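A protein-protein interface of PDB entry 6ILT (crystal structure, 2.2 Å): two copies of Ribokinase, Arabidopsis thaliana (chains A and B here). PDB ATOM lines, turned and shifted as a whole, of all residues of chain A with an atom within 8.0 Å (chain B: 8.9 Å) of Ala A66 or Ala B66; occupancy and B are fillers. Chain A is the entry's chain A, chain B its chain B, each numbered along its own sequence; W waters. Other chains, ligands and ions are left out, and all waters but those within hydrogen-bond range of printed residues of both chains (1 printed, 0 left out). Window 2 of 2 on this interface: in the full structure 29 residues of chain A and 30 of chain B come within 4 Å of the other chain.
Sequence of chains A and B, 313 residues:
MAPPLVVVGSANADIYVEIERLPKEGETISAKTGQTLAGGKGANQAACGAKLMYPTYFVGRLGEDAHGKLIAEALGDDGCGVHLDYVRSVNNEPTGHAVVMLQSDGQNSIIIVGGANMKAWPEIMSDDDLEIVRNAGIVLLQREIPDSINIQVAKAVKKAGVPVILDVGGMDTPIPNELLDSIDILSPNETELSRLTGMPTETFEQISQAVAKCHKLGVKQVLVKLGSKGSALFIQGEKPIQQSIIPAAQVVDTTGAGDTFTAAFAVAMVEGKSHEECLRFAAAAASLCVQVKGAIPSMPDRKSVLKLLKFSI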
ATOM      1  N   ALA A  13       9.849   2.569 -28.806  1.00  0.00           N
ATOM      2  CA  ALA A  13       8.892   3.176 -27.902  1.00  0.00           C
ATOM      3  C   ALA A  13       9.597   3.337 -26.568  1.00  0.00           C
ATOM      4  O   ALA A  13      10.051   2.353 -25.987  1.00  0.00           O
ATOM      5  CB  ALA A  13       7.628   2.326 -27.768  1.00  0.00           C
ATOM      6  N   THR A  36       4.386   7.066 -22.761  1.00  0.00           N
ATOM      7  CA  THR A  36       5.071   6.235 -23.734  1.00  0.00           C
ATOM      8  C   THR A  36       5.270   7.044 -24.996  1.00  0.00           C
ATOM      9  O   THR A  36       4.305   7.456 -25.637  1.00  0.00           O
ATOM     10  CB  THR A  36       4.287   4.947 -24.043  1.00  0.00           C
ATOM     11  OG1 THR A  36       4.249   4.118 -22.876  1.00  0.00           O
ATOM     12  CG2 THR A  36       4.957   4.182 -25.178  1.00  0.00           C
ATOM     13  N   GLY A  63       7.935  -3.868 -35.269  1.00  0.00           N
ATOM     14  CA  GLY A  63       6.999  -4.960 -35.111  1.00  0.00           C
ATOM     15  C   GLY A  63       5.652  -4.477 -35.627  1.00  0.00           C
ATOM     16  O   GLY A  63       5.400  -3.269 -35.669  1.00  0.00           O
ATOM     17  N   GLU A  64       4.790  -5.402 -36.035  1.00  0.00           N
ATOM     18  CA  GLU A  64       3.405  -5.055 -36.351  1.00  0.00           C
ATOM     19  C   GLU A  64       2.608  -5.052 -35.053  1.00  0.00           C
ATOM     20  O   GLU A  64       2.009  -6.062 -34.675  1.00  0.00           O
ATOM     21  CB  GLU A  64       2.807  -6.031 -37.362  1.00  0.00           C
ATOM     22  CG  GLU A  64       3.547  -6.028 -38.676  1.00  0.00           C
ATOM     23  CD  GLU A  64       2.950  -6.960 -39.701  1.00  0.00           C
ATOM     24  OE1 GLU A  64       2.854  -8.173 -39.407  1.00  0.00           O
ATOM     25  OE2 GLU A  64       2.593  -6.480 -40.803  1.00  0.00           O
ATOM     26  N   ASP A  65       2.627  -3.915 -34.363  1.00  0.00           N
ATOM     27  CA  ASP A  65       2.106  -3.825 -33.000  1.00  0.00           C
ATOM     28  C   ASP A  65       1.904  -2.351 -32.664  1.00  0.00           C
ATOM     29  O   ASP A  65       2.287  -1.491 -33.455  1.00  0.00           O
ATOM     30  CB  ASP A  65       3.061  -4.499 -32.002  1.00  0.00           C
ATOM     31  CG  ASP A  65       4.481  -3.902 -32.042  1.00  0.00           C
ATOM     32  OD1 ASP A  65       4.717  -3.038 -32.915  1.00  0.00           O
ATOM     33  OD2 ASP A  65       5.351  -4.296 -31.211  1.00  0.00           O
ATOM     34  N   ALA A  66       1.322  -2.067 -31.502  1.00  0.00           N
ATOM     35  CA  ALA A  66       0.974  -0.699 -31.109  1.00  0.00           C
ATOM     36  C   ALA A  66       2.163   0.255 -31.155  1.00  0.00           C
ATOM     37  O   ALA A  66       2.038   1.369 -31.659  1.00  0.00           O
ATOM     38  CB  ALA A  66       0.371  -0.688 -29.720  1.00  0.00           C
ATOM     39  N   HIS A  67       3.308  -0.173 -30.631  1.00  0.00           N
ATOM     40  CA  HIS A  67       4.496   0.684 -30.616  1.00  0.00           C
ATOM     41  C   HIS A  67       4.962   0.989 -32.028  1.00  0.00           C
ATOM     42  O   HIS A  67       5.358   2.115 -32.338  1.00  0.00           O
ATOM     43  CB  HIS A  67       5.604   0.025 -29.821  1.00  0.00           C
ATOM     44  CG  HIS A  67       5.260  -0.166 -28.386  1.00  0.00           C
ATOM     45  ND1 HIS A  67       5.876  -1.105 -27.588  1.00  0.00           N
ATOM     46  CD2 HIS A  67       4.359   0.465 -27.597  1.00  0.00           C
ATOM     47  CE1 HIS A  67       5.378  -1.039 -26.368  1.00  0.00           C
ATOM     48  NE2 HIS A  67       4.453  -0.094 -26.347  1.00  0.00           N
ATOM     49  N   GLY A  68       4.896  -0.022 -32.881  1.00  0.00           N
ATOM     50  CA  GLY A  68       5.135   0.158 -34.295  1.00  0.00           C
ATOM     51  C   GLY A  68       4.262   1.271 -34.841  1.00  0.00           C
ATOM     52  O   GLY A  68       4.764   2.188 -35.490  1.00  0.00           O
ATOM     53  N   LYS A  69       2.957   1.175 -34.578  1.00  0.00           N
ATOM     54  CA  LYS A  69       1.968   2.186 -34.970  1.00  0.00           C
ATOM     55  C   LYS A  69       2.328   3.558 -34.422  1.00  0.00           C
ATOM     56  O   LYS A  69       2.244   4.578 -35.121  1.00  0.00           O
ATOM     57  CB  LYS A  69       0.571   1.782 -34.467  1.00  0.00           C
ATOM     58  N   LEU A  70       2.735   3.570 -33.156  1.00  0.00           N
ATOM     59  CA  LEU A  70       3.135   4.803 -32.485  1.00  0.00           C
ATOM     60  C   LEU A  70       4.314   5.488 -33.196  1.00  0.00           C
ATOM     61  O   LEU A  70       4.330   6.711 -33.329  1.00  0.00           O
ATOM     62  CB  LEU A  70       3.500   4.520 -31.027  1.00  0.00           C
ATOM     63  CG  LEU A  70       4.113   5.717 -30.306  1.00  0.00           C
ATOM     64  CD1 LEU A  70       3.031   6.695 -29.919  1.00  0.00           C
ATOM     65  CD2 LEU A  70       4.948   5.294 -29.093  1.00  0.00           C
ATOM     66  N   ILE A  71       5.296   4.706 -33.651  1.00  0.00           N
ATOM     67  CA  ILE A  71       6.471   5.308 -34.265  1.00  0.00           C
ATOM     68  C   ILE A  71       6.080   5.914 -35.612  1.00  0.00           C
ATOM     69  O   ILE A  71       6.407   7.060 -35.894  1.00  0.00           O
ATOM     70  CB  ILE A  71       7.628   4.306 -34.483  1.00  0.00           C
ATOM     71  CG1 ILE A  71       7.976   3.558 -33.192  1.00  0.00           C
ATOM     72  CG2 ILE A  71       8.859   5.049 -35.049  1.00  0.00           C
ATOM     73  CD1 ILE A  71       8.386   4.457 -32.048  1.00  0.00           C
ATOM     74  N   ALA A  72       5.357   5.157 -36.437  1.00  0.00           N
ATOM     75  CA  ALA A  72       5.020   5.655 -37.768  1.00  0.00           C
ATOM     76  C   ALA A  72       4.113   6.884 -37.716  1.00  0.00           C
ATOM     77  O   ALA A  72       4.182   7.733 -38.587  1.00  0.00           O
ATOM     78  CB  ALA A  72       4.367   4.569 -38.591  1.00  0.00           C
ATOM     79  N   GLU A  73       3.250   6.964 -36.707  1.00  0.00           N
ATOM     80  CA  GLU A  73       2.316   8.076 -36.617  1.00  0.00           C
ATOM     81  C   GLU A  73       3.108   9.326 -36.318  1.00  0.00           C
ATOM     82  O   GLU A  73       2.923  10.358 -36.965  1.00  0.00           O
ATOM     83  CB  GLU A  73       1.252   7.831 -35.546  1.00  0.00           C
ATOM     84  N   THR A  95       8.295  -4.360 -31.767  1.00  0.00           N
ATOM     85  CA  THR A  95       8.948  -3.083 -31.953  1.00  0.00           C
ATOM     86  C   THR A  95       9.906  -2.869 -30.791  1.00  0.00           C
ATOM     87  O   THR A  95       9.614  -3.247 -29.660  1.00  0.00           O
ATOM     88  CB  THR A  95       7.921  -1.961 -32.046  1.00  0.00           C
ATOM     89  OG1 THR A  95       7.182  -2.142 -33.256  1.00  0.00           O
ATOM     90  CG2 THR A  95       8.599  -0.559 -32.062  1.00  0.00           C
ATOM     91  N   ALA B  13      -2.625  -1.664 -21.479  1.00  0.00           N
ATOM     92  CA  ALA B  13      -1.583  -2.284 -22.284  1.00  0.00           C
ATOM     93  C   ALA B  13      -0.684  -3.058 -21.323  1.00  0.00           C
ATOM     94  O   ALA B  13      -0.124  -2.492 -20.378  1.00  0.00           O
ATOM     95  CB  ALA B  13      -0.790  -1.253 -23.069  1.00  0.00           C
ATOM     96  N   ILE B  15       2.689  -4.683 -20.862  1.00  0.00           N
ATOM     97  CA  ILE B  15       4.047  -4.651 -21.420  1.00  0.00           C
ATOM     98  C   ILE B  15       4.944  -5.677 -20.755  1.00  0.00           C
ATOM     99  O   ILE B  15       5.465  -5.429 -19.671  1.00  0.00           O
ATOM    100  CB  ILE B  15       4.730  -3.280 -21.225  1.00  0.00           C
ATOM    101  CG1 ILE B  15       3.752  -2.135 -21.433  1.00  0.00           C
ATOM    102  CG2 ILE B  15       5.944  -3.151 -22.134  1.00  0.00           C
ATOM    103  CD1 ILE B  15       3.199  -2.120 -22.780  1.00  0.00           C
ATOM    104  N   GLN B  35       6.867  -8.261 -25.189  1.00  0.00           N
ATOM    105  CA  GLN B  35       5.630  -8.181 -25.940  1.00  0.00           C
ATOM    106  C   GLN B  35       4.587  -7.371 -25.187  1.00  0.00           C
ATOM    107  O   GLN B  35       4.447  -7.463 -23.964  1.00  0.00           O
ATOM    108  CB  GLN B  35       5.083  -9.561 -26.255  1.00  0.00           C
ATOM    109  CG  GLN B  35       4.264  -9.560 -27.529  1.00  0.00           C
ATOM    110  CD  GLN B  35       3.525 -10.864 -27.740  1.00  0.00           C
ATOM    111  OE1 GLN B  35       3.677 -11.807 -26.963  1.00  0.00           O
ATOM    112  NE2 GLN B  35       2.710 -10.923 -28.790  1.00  0.00           N
ATOM    113  N   THR B  36       3.872  -6.564 -25.948  1.00  0.00           N
ATOM    114  CA  THR B  36       2.835  -5.719 -25.425  1.00  0.00           C
ATOM    115  C   THR B  36       1.507  -6.308 -25.830  1.00  0.00           C
ATOM    116  O   THR B  36       1.301  -6.600 -27.000  1.00  0.00           O
ATOM    117  CB  THR B  36       2.950  -4.303 -25.947  1.00  0.00           C
ATOM    118  OG1 THR B  36       4.046  -3.671 -25.291  1.00  0.00           O
ATOM    119  CG2 THR B  36       1.676  -3.526 -25.626  1.00  0.00           C
ATOM    120  N   LEU B  37       0.617  -6.514 -24.865  1.00  0.00           N
ATOM    121  CA  LEU B  37      -0.697  -7.078 -25.174  1.00  0.00           C
ATOM    122  C   LEU B  37      -1.834  -6.247 -24.594  1.00  0.00           C
ATOM    123  O   LEU B  37      -1.686  -5.612 -23.543  1.00  0.00           O
ATOM    124  CB  LEU B  37      -0.791  -8.507 -24.651  1.00  0.00           C
ATOM    125  CG  LEU B  37      -0.134  -9.576 -25.526  1.00  0.00           C
ATOM    126  CD1 LEU B  37       1.373  -9.590 -25.336  1.00  0.00           C
ATOM    127  CD2 LEU B  37      -0.738 -10.947 -25.246  1.00  0.00           C
ATOM    128  N   ALA B  38      -2.960  -6.238 -25.295  1.00  0.00           N
ATOM    129  CA  ALA B  38      -4.192  -5.715 -24.735  1.00  0.00           C
ATOM    130  C   ALA B  38      -4.629  -6.598 -23.565  1.00  0.00           C
ATOM    131  O   ALA B  38      -4.808  -7.808 -23.719  1.00  0.00           O
ATOM    132  CB  ALA B  38      -5.278  -5.657 -25.791  1.00  0.00           C
ATOM    133  N   LEU B  62     -10.145   5.147 -21.832  1.00  0.00           N
ATOM    134  CA  LEU B  62      -8.866   5.081 -22.530  1.00  0.00           C
ATOM    135  C   LEU B  62      -8.284   6.473 -22.701  1.00  0.00           C
ATOM    136  O   LEU B  62      -9.019   7.456 -22.690  1.00  0.00           O
ATOM    137  CB  LEU B  62      -9.024   4.459 -23.919  1.00  0.00           C
ATOM    138  CG  LEU B  62      -9.723   3.113 -24.029  1.00  0.00           C
ATOM    139  CD1 LEU B  62      -9.919   2.772 -25.494  1.00  0.00           C
ATOM    140  CD2 LEU B  62      -8.917   2.044 -23.302  1.00  0.00           C
ATOM    141  N   GLY B  63      -6.967   6.552 -22.872  1.00  0.00           N
ATOM    142  CA  GLY B  63      -6.333   7.761 -23.380  1.00  0.00           C
ATOM    143  C   GLY B  63      -6.374   7.761 -24.900  1.00  0.00           C
ATOM    144  O   GLY B  63      -6.580   6.716 -25.531  1.00  0.00           O
ATOM    145  N   GLU B  64      -6.205   8.926 -25.510  1.00  0.00           N
ATOM    146  CA  GLU B  64      -6.233   8.981 -26.968  1.00  0.00           C
ATOM    147  C   GLU B  64      -4.820   8.771 -27.506  1.00  0.00           C
ATOM    148  O   GLU B  64      -4.255   9.629 -28.173  1.00  0.00           O
ATOM    149  CB  GLU B  64      -6.833  10.303 -27.440  1.00  0.00           C
ATOM    150  CG  GLU B  64      -8.024  10.701 -26.596  1.00  0.00           C
ATOM    151  CD  GLU B  64      -9.088  11.469 -27.351  1.00  0.00           C
ATOM    152  OE1 GLU B  64      -8.850  11.849 -28.522  1.00  0.00           O
ATOM    153  OE2 GLU B  64     -10.160  11.708 -26.751  1.00  0.00           O
ATOM    154  N   ASP B  65      -4.267   7.604 -27.196  1.00  0.00           N
ATOM    155  CA  ASP B  65      -2.914   7.250 -27.573  1.00  0.00           C
ATOM    156  C   ASP B  65      -2.902   5.905 -28.299  1.00  0.00           C
ATOM    157  O   ASP B  65      -3.957   5.360 -28.647  1.00  0.00           O
ATOM    158  CB  ASP B  65      -2.003   7.219 -26.339  1.00  0.00           C
ATOM    159  CG  ASP B  65      -2.592   6.408 -25.182  1.00  0.00           C
ATOM    160  OD1 ASP B  65      -3.427   5.506 -25.422  1.00  0.00           O
ATOM    161  OD2 ASP B  65      -2.209   6.669 -24.026  1.00  0.00           O
ATOM    162  N   ALA B  66      -1.705   5.380 -28.531  1.00  0.00           N
ATOM    163  CA  ALA B  66      -1.544   4.131 -29.261  1.00  0.00           C
ATOM    164  C   ALA B  66      -2.072   2.936 -28.458  1.00  0.00           C
ATOM    165  O   ALA B  66      -2.789   2.067 -28.983  1.00  0.00           O
ATOM    166  CB  ALA B  66      -0.073   3.930 -29.610  1.00  0.00           C
ATOM    167  N   HIS B  67      -1.687   2.883 -27.189  1.00  0.00           N
ATOM    168  CA  HIS B  67      -2.168   1.828 -26.289  1.00  0.00           C
ATOM    169  C   HIS B  67      -3.692   1.807 -26.312  1.00  0.00           C
ATOM    170  O   HIS B  67      -4.294   0.747 -26.394  1.00  0.00           O
ATOM    171  CB  HIS B  67      -1.640   2.039 -24.868  1.00  0.00           C
ATOM    172  CG  HIS B  67      -0.178   1.739 -24.715  1.00  0.00           C
ATOM    173  ND1 HIS B  67       0.576   2.210 -23.658  1.00  0.00           N
ATOM    174  CD2 HIS B  67       0.670   1.015 -25.486  1.00  0.00           C
ATOM    175  CE1 HIS B  67       1.826   1.797 -23.788  1.00  0.00           C
ATOM    176  NE2 HIS B  67       1.906   1.060 -24.884  1.00  0.00           N
ATOM    177  N   GLY B  68      -4.303   2.994 -26.304  1.00  0.00           N
ATOM    178  CA  GLY B  68      -5.746   3.124 -26.411  1.00  0.00           C
ATOM    179  C   GLY B  68      -6.342   2.449 -27.636  1.00  0.00           C
ATOM    180  O   GLY B  68      -7.338   1.726 -27.539  1.00  0.00           O
ATOM    181  N   LYS B  69      -5.719   2.665 -28.790  1.00  0.00           N
ATOM    182  CA  LYS B  69      -6.227   2.128 -30.053  1.00  0.00           C
ATOM    183  C   LYS B  69      -6.002   0.625 -30.127  1.00  0.00           C
ATOM    184  O   LYS B  69      -6.818  -0.107 -30.704  1.00  0.00           O
ATOM    185  CB  LYS B  69      -5.555   2.826 -31.246  1.00  0.00           C
ATOM    186  N   LEU B  70      -4.889   0.172 -29.547  1.00  0.00           N
ATOM    187  CA  LEU B  70      -4.622  -1.267 -29.369  1.00  0.00           C
ATOM    188  C   LEU B  70      -5.796  -1.968 -28.671  1.00  0.00           C
ATOM    189  O   LEU B  70      -6.281  -3.000 -29.134  1.00  0.00           O
ATOM    190  CB  LEU B  70      -3.337  -1.487 -28.559  1.00  0.00           C
ATOM    191  CG  LEU B  70      -3.031  -2.891 -28.032  1.00  0.00           C
ATOM    192  CD1 LEU B  70      -2.695  -3.821 -29.186  1.00  0.00           C
ATOM    193  CD2 LEU B  70      -1.905  -2.890 -26.997  1.00  0.00           C
ATOM    194  N   ILE B  71      -6.253  -1.389 -27.566  1.00  0.00           N
ATOM    195  CA  ILE B  71      -7.374  -1.962 -26.825  1.00  0.00           C
ATOM    196  C   ILE B  71      -8.618  -2.022 -27.714  1.00  0.00           C
ATOM    197  O   ILE B  71      -9.215  -3.091 -27.911  1.00  0.00           O
ATOM    198  CB  ILE B  71      -7.705  -1.143 -25.554  1.00  0.00           C
ATOM    199  CG1 ILE B  71      -6.440  -0.818 -24.751  1.00  0.00           C
ATOM    200  CG2 ILE B  71      -8.720  -1.886 -24.691  1.00  0.00           C
ATOM    201  CD1 ILE B  71      -5.836  -1.991 -24.105  1.00  0.00           C
ATOM    202  N   ALA B  72      -9.000  -0.866 -28.254  1.00  0.00           N
ATOM    203  CA  ALA B  72     -10.189  -0.781 -29.085  1.00  0.00           C
ATOM    204  C   ALA B  72     -10.126  -1.779 -30.229  1.00  0.00           C
ATOM    205  O   ALA B  72     -11.111  -2.465 -30.528  1.00  0.00           O
ATOM    206  CB  ALA B  72     -10.357   0.625 -29.618  1.00  0.00           C
ATOM    207  N   GLU B  73      -8.952  -1.886 -30.841  1.00  0.00           N
ATOM    208  CA  GLU B  73      -8.766  -2.808 -31.954  1.00  0.00           C
ATOM    209  C   GLU B  73      -9.034  -4.234 -31.512  1.00  0.00           C
ATOM    210  O   GLU B  73      -9.813  -4.943 -32.145  1.00  0.00           O
ATOM    211  CB  GLU B  73      -7.354  -2.688 -32.536  1.00  0.00           C
ATOM    212  N   ALA B  74      -8.402  -4.651 -30.420  1.00  0.00           N
ATOM    213  CA  ALA B  74      -8.592  -6.006 -29.915  1.00  0.00           C
ATOM    214  C   ALA B  74     -10.064  -6.322 -29.560  1.00  0.00           C
ATOM    215  O   ALA B  74     -10.596  -7.392 -29.907  1.00  0.00           O
ATOM    216  CB  ALA B  74      -7.689  -6.230 -28.698  1.00  0.00           C
ATOM    217  N   GLU B  93      -4.976  12.013 -20.093  1.00  0.00           N
ATOM    218  CA  GLU B  93      -4.474  10.823 -19.406  1.00  0.00           C
ATOM    219  C   GLU B  93      -4.077   9.735 -20.399  1.00  0.00           C
ATOM    220  O   GLU B  93      -4.739   9.551 -21.415  1.00  0.00           O
ATOM    221  CB  GLU B  93      -5.522  10.273 -18.420  1.00  0.00           C
ATOM    222  CG  GLU B  93      -5.824  11.179 -17.213  1.00  0.00           C
ATOM    223  CD  GLU B  93      -4.651  11.331 -16.236  1.00  0.00           C
ATOM    224  OE1 GLU B  93      -3.574  10.724 -16.441  1.00  0.00           O
ATOM    225  OE2 GLU B  93      -4.815  12.068 -15.242  1.00  0.00           O
ATOM    226  N   PRO B  94      -2.988   9.010 -20.109  1.00  0.00           N
ATOM    227  CA  PRO B  94      -2.649   7.867 -20.964  1.00  0.00           C
ATOM    228  C   PRO B  94      -3.543   6.665 -20.637  1.00  0.00           C
ATOM    229  O   PRO B  94      -4.065   6.558 -19.523  1.00  0.00           O
ATOM    230  CB  PRO B  94      -1.193   7.583 -20.598  1.00  0.00           C
ATOM    231  CG  PRO B  94      -1.137   7.938 -19.122  1.00  0.00           C
ATOM    232  CD  PRO B  94      -2.099   9.109 -18.937  1.00  0.00           C
ATOM    233  N   THR B  95      -3.733   5.791 -21.612  1.00  0.00           N
ATOM    234  CA  THR B  95      -4.320   4.496 -21.373  1.00  0.00           C
ATOM    235  C   THR B  95      -3.529   3.782 -20.288  1.00  0.00           C
ATOM    236  O   THR B  95      -2.312   3.835 -20.275  1.00  0.00           O
ATOM    237  CB  THR B  95      -4.345   3.684 -22.647  1.00  0.00           C
ATOM    238  OG1 THR B  95      -5.116   4.405 -23.614  1.00  0.00           O
ATOM    239  CG2 THR B  95      -4.976   2.295 -22.405  1.00  0.00           C
ATOM    240  N   GLY B  96      -4.218   3.147 -19.348  1.00  0.00           N
ATOM    241  CA  GLY B  96      -3.530   2.411 -18.301  1.00  0.00           C
ATOM    242  C   GLY B  96      -2.552   1.413 -18.891  1.00  0.00           C
ATOM    243  O   GLY B  96      -2.753   0.876 -19.984  1.00  0.00           O
HETATM  244  O   HOH W   1       4.845  -6.390 -28.862  1.00  0.00           O
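Printed residues of chain B within 4 Å of Thr A36: His B67 (3.5 Å).
Ala A66 touches just these residues of chain B: Ala B66 and Leu B70.
Printed residues of chain B within 4 Å of His A67: Thr B36 and His B67.
No residue of chain B comes within 4 Å of Gly A68.
No residue of chain B comes within 4 Å of Lys A69.
Ala B13 touches none of the printed residues of chain A.
Glu B64 touches none of the printed residues of chain A.
Of chain A, only Ala A66 and Leu A70 come within 4 Å of Ala B66.
Printed residues of chain A within 4 Å of His B67: Thr A36 and His A67.
Of the printed residues of chain A, Leu B70 touches Ala A66.
The nearest residue of chain B that does not touch Ala A66 is His B67 (4.6 Å).
The nearest residue of chain A that does not touch Ala B66 is Lys A69 (5.3 Å).
The nearest printed residue of chain A that does not touch Leu B70 is Asp A65 (6.0 Å).
Water W1 lies within hydrogen-bond range of the backbone NH (N) of Thr B36 (3.1 Å) and the side-chain carboxylate (OD2) of Asp A65 (3.2 Å).
Printed residues of chain B that touch a printed residue of chain A: Thr B36, Ala B66, His B67 and Leu B70.
Among the printed residues, 6 pairs touch across the chains.
Among the printed residues, no Asp or Glu carboxylate lies within 4 Å of a Lys or Arg side-chain nitrogen of the other chain.
Among the printed residues, merely in contact across the chains: His A67 with Thr B36 (3.1 Å), Thr A36 with His B67 (3.5 Å), Leu A70 with Ala B66 (3.9 Å), Ala A66 with Ala B66 (3.9 Å) and Ala A66 with Leu B70 (3.97 Å).
Thr A36 touches His B67, and with the chains exchanged His A67 touches Thr B36.
Ala A66 touches its own counterpart, Ala B66.
Ala A66 touches Leu B70, and with the chains exchanged Leu A70 touches Ala B66.
His A67 touches its own counterpart, His B67.
Of the 6 pairs that touch across the chains among the printed residues, 6 have their exchanged pair printed and touching as well.
A ring nitrogen (NE2) of His B67 sits at hydrogen-bond distance from a ring nitrogen (NE2) of His A67 (3.2 Å).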
